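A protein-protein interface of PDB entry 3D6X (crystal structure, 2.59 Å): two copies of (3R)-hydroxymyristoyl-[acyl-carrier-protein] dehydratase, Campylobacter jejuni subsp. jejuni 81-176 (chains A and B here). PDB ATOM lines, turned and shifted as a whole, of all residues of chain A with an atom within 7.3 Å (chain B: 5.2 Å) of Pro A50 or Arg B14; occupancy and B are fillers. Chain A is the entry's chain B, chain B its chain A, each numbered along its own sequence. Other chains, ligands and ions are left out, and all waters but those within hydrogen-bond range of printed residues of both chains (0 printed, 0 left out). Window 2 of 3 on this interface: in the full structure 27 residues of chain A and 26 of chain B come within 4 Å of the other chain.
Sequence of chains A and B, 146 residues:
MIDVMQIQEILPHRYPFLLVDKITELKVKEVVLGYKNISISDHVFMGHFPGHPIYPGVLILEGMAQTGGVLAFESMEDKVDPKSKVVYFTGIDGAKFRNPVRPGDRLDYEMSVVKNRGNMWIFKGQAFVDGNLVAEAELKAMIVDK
The backbone carbonyl oxygen (O) of Gly A47 lies within hydrogen-bond range of the backbone NH (N) of Arg B14, 3.0 Å away.
The backbone carbonyl oxygen (O) of Leu B11 lies within hydrogen-bond range of the guanidinium group (NH2) of Arg B14 (3.0 Å). The backbone carbonyl oxygen (O) of Gln B8 is in hydrogen-bond range of the guanidinium group (NH1) of Arg B14, 2.8 Å away.
Among the printed residues, pairs that only touch across the chains: Val A44 with Phe B17 (3.8 Å), Met A46 with Pro B16 (3.7 Å), Gly A47 with His B13 (3.8 Å), Gly A47 with Tyr B15 (3.4 Å), Gly A47 with Pro B16 (3.7 Å), His A48 with Phe B17 (3.7 Å), Phe A49 with Pro B12 (3.5 Å), Phe A49 with His B13 (3.6 Å) and Pro A50 with Arg B14 (3.9 Å).
Printed residues of chain B within 4 Å of Val A44: Phe B17 (3.8 Å). Printed residues of chain B within 4 Å of Met A46: Pro B16 (3.7 Å). Of the printed residues of chain B, Gly A47 touches His B13, Arg B14, Tyr B15 and Pro B16. Of the printed residues of chain B, Phe A49 touches Pro B12 (3.5 Å) and His B13 (3.6 Å). Pro A50 touches one residue of chain B. Pro A53 touches none of the printed residues of chain B. Gln B8 touches none of the printed residues of chain A. Of chain A, only Gly A47 and Pro A50 come within 4 Å of Arg B14. Printed residues of chain A within 4 Å of Pro B16: Met A46 (3.7 Å) and Gly A47 (3.7 Å). The nearest residue of chain B that does not touch Pro A50 is Pro B12 (4.2 Å).
Hydrophobic or aromatic side chains of chain B within 4 Å of the printed part of chain A: Pro B12, His B13, Pro B16 and Phe B17. Of the 10 printed residues of chain A, 6 touch a printed residue of chain B. Printed residues of chain A that touch a printed residue of chain B: Val A44, Met A46, Gly A47, His A48, Phe A49 and Pro A50.
No position is printed for both chains.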
ATOM      1  N   VAL A  44     -28.112  34.731 -23.644  1.00  0.00           N
ATOM      2  CA  VAL A  44     -27.614  34.321 -22.310  1.00  0.00           C
ATOM      3  C   VAL A  44     -27.870  32.871 -22.006  1.00  0.00           C
ATOM      4  O   VAL A  44     -27.063  32.245 -21.334  1.00  0.00           O
ATOM      5  CB  VAL A  44     -28.126  35.117 -21.054  1.00  0.00           C
ATOM      6  CG1 VAL A  44     -27.187  36.187 -20.733  1.00  0.00           C
ATOM      7  CG2 VAL A  44     -29.478  35.681 -21.211  1.00  0.00           C
ATOM      8  N   PHE A  45     -28.998  32.344 -22.458  1.00  0.00           N
ATOM      9  CA  PHE A  45     -29.378  31.016 -22.032  1.00  0.00           C
ATOM     10  C   PHE A  45     -28.515  29.950 -22.685  1.00  0.00           C
ATOM     11  O   PHE A  45     -28.462  28.820 -22.214  1.00  0.00           O
ATOM     12  CB  PHE A  45     -30.856  30.742 -22.265  1.00  0.00           C
ATOM     13  CG  PHE A  45     -31.763  31.632 -21.475  1.00  0.00           C
ATOM     14  CD1 PHE A  45     -32.560  32.568 -22.108  1.00  0.00           C
ATOM     15  CD2 PHE A  45     -31.818  31.545 -20.097  1.00  0.00           C
ATOM     16  CE1 PHE A  45     -33.416  33.394 -21.381  1.00  0.00           C
ATOM     17  CE2 PHE A  45     -32.668  32.376 -19.357  1.00  0.00           C
ATOM     18  CZ  PHE A  45     -33.471  33.296 -20.010  1.00  0.00           C
ATOM     19  N   MET A  46     -27.814  30.296 -23.755  1.00  0.00           N
ATOM     20  CA  MET A  46     -26.809  29.363 -24.293  1.00  0.00           C
ATOM     21  C   MET A  46     -25.903  28.803 -23.203  1.00  0.00           C
ATOM     22  O   MET A  46     -25.588  27.621 -23.184  1.00  0.00           O
ATOM     23  CB  MET A  46     -25.882  30.067 -25.268  1.00  0.00           C
ATOM     24  CG  MET A  46     -26.256  29.960 -26.691  1.00  0.00           C
ATOM     25  SD  MET A  46     -24.611  30.201 -27.718  1.00  0.00           S
ATOM     26  CE  MET A  46     -24.644  32.187 -27.875  1.00  0.00           C
ATOM     27  N   GLY A  47     -25.481  29.678 -22.300  1.00  0.00           N
ATOM     28  CA  GLY A  47     -24.409  29.389 -21.373  1.00  0.00           C
ATOM     29  C   GLY A  47     -24.819  29.579 -19.930  1.00  0.00           C
ATOM     30  O   GLY A  47     -24.157  29.062 -19.043  1.00  0.00           O
ATOM     31  N   HIS A  48     -25.903  30.318 -19.682  1.00  0.00           N
ATOM     32  CA  HIS A  48     -26.428  30.363 -18.325  1.00  0.00           C
ATOM     33  C   HIS A  48     -27.393  29.231 -18.159  1.00  0.00           C
ATOM     34  O   HIS A  48     -28.593  29.391 -17.885  1.00  0.00           O
ATOM     35  CB  HIS A  48     -27.040  31.679 -17.896  1.00  0.00           C
ATOM     36  CG  HIS A  48     -26.914  31.911 -16.422  1.00  0.00           C
ATOM     37  ND1 HIS A  48     -28.001  31.991 -15.580  1.00  0.00           N
ATOM     38  CD2 HIS A  48     -25.822  32.044 -15.639  1.00  0.00           C
ATOM     39  CE1 HIS A  48     -27.586  32.182 -14.342  1.00  0.00           C
ATOM     40  NE2 HIS A  48     -26.267  32.206 -14.349  1.00  0.00           N
ATOM     41  N   PHE A  49     -26.772  28.093 -18.430  1.00  0.00           N
ATOM     42  CA  PHE A  49     -27.081  26.747 -18.003  1.00  0.00           C
ATOM     43  C   PHE A  49     -27.720  25.992 -19.125  1.00  0.00           C
ATOM     44  O   PHE A  49     -28.916  26.078 -19.328  1.00  0.00           O
ATOM     45  CB  PHE A  49     -27.808  26.698 -16.668  1.00  0.00           C
ATOM     46  CG  PHE A  49     -27.109  27.480 -15.606  1.00  0.00           C
ATOM     47  CD1 PHE A  49     -27.811  28.257 -14.701  1.00  0.00           C
ATOM     48  CD2 PHE A  49     -25.731  27.493 -15.554  1.00  0.00           C
ATOM     49  CE1 PHE A  49     -27.151  28.985 -13.762  1.00  0.00           C
ATOM     50  CE2 PHE A  49     -25.073  28.241 -14.606  1.00  0.00           C
ATOM     51  CZ  PHE A  49     -25.785  28.973 -13.718  1.00  0.00           C
ATOM     52  N   PRO A  50     -26.871  25.329 -19.912  1.00  0.00           N
ATOM     53  CA  PRO A  50     -27.197  24.286 -20.843  1.00  0.00           C
ATOM     54  C   PRO A  50     -28.177  23.338 -20.179  1.00  0.00           C
ATOM     55  O   PRO A  50     -27.861  22.784 -19.116  1.00  0.00           O
ATOM     56  CB  PRO A  50     -25.854  23.569 -21.022  1.00  0.00           C
ATOM     57  CG  PRO A  50     -24.858  24.643 -20.913  1.00  0.00           C
ATOM     58  CD  PRO A  50     -25.431  25.633 -19.920  1.00  0.00           C
ATOM     59  N   GLY A  51     -29.346  23.155 -20.800  1.00  0.00           N
ATOM     60  CA  GLY A  51     -30.388  22.306 -20.244  1.00  0.00           C
ATOM     61  C   GLY A  51     -31.067  22.863 -18.997  1.00  0.00           C
ATOM     62  O   GLY A  51     -31.893  22.192 -18.395  1.00  0.00           O
ATOM     63  N   HIS A  52     -30.719  24.081 -18.592  1.00  0.00           N
ATOM     64  CA  HIS A  52     -31.414  24.735 -17.472  1.00  0.00           C
ATOM     65  C   HIS A  52     -31.428  26.275 -17.572  1.00  0.00           C
ATOM     66  O   HIS A  52     -30.683  26.982 -16.893  1.00  0.00           O
ATOM     67  CB  HIS A  52     -30.832  24.284 -16.130  1.00  0.00           C
ATOM     68  CG  HIS A  52     -31.719  24.579 -14.953  1.00  0.00           C
ATOM     69  ND1 HIS A  52     -31.260  25.183 -13.798  1.00  0.00           N
ATOM     70  CD2 HIS A  52     -33.041  24.343 -14.750  1.00  0.00           C
ATOM     71  CE1 HIS A  52     -32.258  25.305 -12.937  1.00  0.00           C
ATOM     72  NE2 HIS A  52     -33.350  24.800 -13.488  1.00  0.00           N
ATOM     73  N   PRO A  53     -32.282  26.812 -18.422  1.00  0.00           N
ATOM     74  CA  PRO A  53     -32.241  28.262 -18.633  1.00  0.00           C
ATOM     75  C   PRO A  53     -32.695  29.079 -17.417  1.00  0.00           C
ATOM     76  O   PRO A  53     -33.850  28.986 -17.006  1.00  0.00           O
ATOM     77  CB  PRO A  53     -33.220  28.469 -19.785  1.00  0.00           C
ATOM     78  CG  PRO A  53     -34.116  27.285 -19.773  1.00  0.00           C
ATOM     79  CD  PRO A  53     -33.346  26.147 -19.190  1.00  0.00           C
ATOM     80  N   GLN B   8     -14.380  24.957 -15.737  1.00  0.00           N
ATOM     81  CA  GLN B   8     -15.575  24.440 -16.388  1.00  0.00           C
ATOM     82  C   GLN B   8     -16.029  23.051 -15.908  1.00  0.00           C
ATOM     83  O   GLN B   8     -17.194  22.695 -16.071  1.00  0.00           O
ATOM     84  CB  GLN B   8     -15.409  24.441 -17.906  1.00  0.00           C
ATOM     85  CG  GLN B   8     -15.708  25.779 -18.573  1.00  0.00           C
ATOM     86  CD  GLN B   8     -15.586  25.663 -20.069  1.00  0.00           C
ATOM     87  OE1 GLN B   8     -16.433  25.050 -20.725  1.00  0.00           O
ATOM     88  NE2 GLN B   8     -14.505  26.196 -20.616  1.00  0.00           N
ATOM     89  N   GLU B   9     -15.118  22.275 -15.328  1.00  0.00           N
ATOM     90  CA  GLU B   9     -15.465  20.973 -14.746  1.00  0.00           C
ATOM     91  C   GLU B   9     -16.148  21.143 -13.372  1.00  0.00           C
ATOM     92  O   GLU B   9     -16.697  20.197 -12.814  1.00  0.00           O
ATOM     93  CB  GLU B   9     -14.204  20.116 -14.634  1.00  0.00           C
ATOM     94  CG  GLU B   9     -14.444  18.617 -14.389  1.00  0.00           C
ATOM     95  CD  GLU B   9     -15.332  17.956 -15.452  1.00  0.00           C
ATOM     96  OE1 GLU B   9     -15.503  18.541 -16.545  1.00  0.00           O
ATOM     97  OE2 GLU B   9     -15.858  16.848 -15.192  1.00  0.00           O
ATOM     98  N   LEU B  11     -17.752  24.674 -12.287  1.00  0.00           N
ATOM     99  CA  LEU B  11     -18.920  25.532 -12.537  1.00  0.00           C
ATOM    100  C   LEU B  11     -19.677  25.013 -13.735  1.00  0.00           C
ATOM    101  O   LEU B  11     -19.068  24.505 -14.671  1.00  0.00           O
ATOM    102  CB  LEU B  11     -18.517  26.982 -12.788  1.00  0.00           C
ATOM    103  CG  LEU B  11     -17.844  27.754 -11.659  1.00  0.00           C
ATOM    104  CD1 LEU B  11     -17.432  29.144 -12.140  1.00  0.00           C
ATOM    105  CD2 LEU B  11     -18.727  27.813 -10.409  1.00  0.00           C
ATOM    106  N   PRO B  12     -21.017  25.137 -13.714  1.00  0.00           N
ATOM    107  CA  PRO B  12     -21.854  24.808 -14.869  1.00  0.00           C
ATOM    108  C   PRO B  12     -21.886  25.921 -15.926  1.00  0.00           C
ATOM    109  O   PRO B  12     -22.344  25.692 -17.034  1.00  0.00           O
ATOM    110  CB  PRO B  12     -23.243  24.690 -14.259  1.00  0.00           C
ATOM    111  CG  PRO B  12     -23.247  25.652 -13.161  1.00  0.00           C
ATOM    112  CD  PRO B  12     -21.836  25.602 -12.579  1.00  0.00           C
ATOM    113  N   HIS B  13     -21.410  27.118 -15.589  1.00  0.00           N
ATOM    114  CA  HIS B  13     -21.502  28.227 -16.518  1.00  0.00           C
ATOM    115  C   HIS B  13     -20.708  27.967 -17.794  1.00  0.00           C
ATOM    116  O   HIS B  13     -19.621  27.379 -17.767  1.00  0.00           O
ATOM    117  CB  HIS B  13     -20.996  29.511 -15.884  1.00  0.00           C
ATOM    118  CG  HIS B  13     -21.563  29.795 -14.529  1.00  0.00           C
ATOM    119  ND1 HIS B  13     -22.030  31.040 -14.169  1.00  0.00           N
ATOM    120  CD2 HIS B  13     -21.707  29.012 -13.440  1.00  0.00           C
ATOM    121  CE1 HIS B  13     -22.438  31.012 -12.917  1.00  0.00           C
ATOM    122  NE2 HIS B  13     -22.253  29.794 -12.452  1.00  0.00           N
ATOM    123  N   ARG B  14     -21.241  28.419 -18.916  1.00  0.00           N
ATOM    124  CA  ARG B  14     -20.552  28.256 -20.185  1.00  0.00           C
ATOM    125  C   ARG B  14     -20.575  29.565 -20.949  1.00  0.00           C
ATOM    126  O   ARG B  14     -21.292  30.496 -20.572  1.00  0.00           O
ATOM    127  CB  ARG B  14     -21.212  27.146 -20.979  1.00  0.00           C
ATOM    128  CG  ARG B  14     -21.172  25.821 -20.270  1.00  0.00           C
ATOM    129  CD  ARG B  14     -19.738  25.306 -20.189  1.00  0.00           C
ATOM    130  NE  ARG B  14     -19.658  23.946 -19.652  1.00  0.00           N
ATOM    131  CZ  ARG B  14     -19.192  23.666 -18.436  1.00  0.00           C
ATOM    132  NH1 ARG B  14     -19.151  22.417 -17.996  1.00  0.00           N
ATOM    133  NH2 ARG B  14     -18.779  24.654 -17.657  1.00  0.00           N
ATOM    134  N   TYR B  15     -19.769  29.663 -21.999  1.00  0.00           N
ATOM    135  CA  TYR B  15     -19.840  30.841 -22.848  1.00  0.00           C
ATOM    136  C   TYR B  15     -21.290  30.943 -23.329  1.00  0.00           C
ATOM    137  O   TYR B  15     -21.906  29.923 -23.653  1.00  0.00           O
ATOM    138  CB  TYR B  15     -18.904  30.677 -24.018  1.00  0.00           C
ATOM    139  CG  TYR B  15     -19.123  31.673 -25.128  1.00  0.00           C
ATOM    140  CD1 TYR B  15     -18.498  32.913 -25.105  1.00  0.00           C
ATOM    141  CD2 TYR B  15     -19.934  31.373 -26.205  1.00  0.00           C
ATOM    142  CE1 TYR B  15     -18.667  33.785 -26.109  1.00  0.00           C
ATOM    143  CE2 TYR B  15     -20.118  32.267 -27.210  1.00  0.00           C
ATOM    144  CZ  TYR B  15     -19.476  33.465 -27.156  1.00  0.00           C
ATOM    145  OH  TYR B  15     -19.641  34.371 -28.159  1.00  0.00           O
ATOM    146  N   PRO B  16     -21.844  32.161 -23.394  1.00  0.00           N
ATOM    147  CA  PRO B  16     -21.268  33.471 -23.189  1.00  0.00           C
ATOM    148  C   PRO B  16     -21.480  34.046 -21.793  1.00  0.00           C
ATOM    149  O   PRO B  16     -21.522  35.257 -21.646  1.00  0.00           O
ATOM    150  CB  PRO B  16     -22.097  34.317 -24.137  1.00  0.00           C
ATOM    151  CG  PRO B  16     -23.451  33.750 -23.985  1.00  0.00           C
ATOM    152  CD  PRO B  16     -23.265  32.269 -23.747  1.00  0.00           C
ATOM    153  N   PHE B  17     -21.611  33.211 -20.769  1.00  0.00           N
ATOM    154  CA  PHE B  17     -21.718  33.755 -19.437  1.00  0.00           C
ATOM    155  C   PHE B  17     -20.702  33.120 -18.465  1.00  0.00           C
ATOM    156  O   PHE B  17     -21.004  32.926 -17.294  1.00  0.00           O
ATOM    157  CB  PHE B  17     -23.177  33.670 -18.948  1.00  0.00           C
ATOM    158  CG  PHE B  17     -23.616  34.864 -18.133  1.00  0.00           C
ATOM    159  CD1 PHE B  17     -23.672  34.804 -16.745  1.00  0.00           C
ATOM    160  CD2 PHE B  17     -23.959  36.069 -18.758  1.00  0.00           C
ATOM    161  CE1 PHE B  17     -24.066  35.899 -16.004  1.00  0.00           C
ATOM    162  CE2 PHE B  17     -24.355  37.194 -18.008  1.00  0.00           C
ATOM    163  CZ  PHE B  17     -24.404  37.098 -16.640  1.00  0.00           C
ATOM    164  N   LEU B  18     -19.508  32.790 -18.964  1.00  0.00           N
ATOM    165  CA  LEU B  18     -18.419  32.286 -18.150  1.00  0.00           C
ATOM    166  C   LEU B  18     -17.426  33.426 -18.041  1.00  0.00           C
ATOM    167  O   LEU B  18     -16.745  33.746 -19.008  1.00  0.00           O
ATOM    168  CB  LEU B  18     -17.793  31.070 -18.819  1.00  0.00           C
ATOM    169  CG  LEU B  18     -16.585  30.355 -18.186  1.00  0.00           C
ATOM    170  CD1 LEU B  18     -16.699  30.106 -16.684  1.00  0.00           C
ATOM    171  CD2 LEU B  18     -16.296  29.051 -18.926  1.00  0.00           C
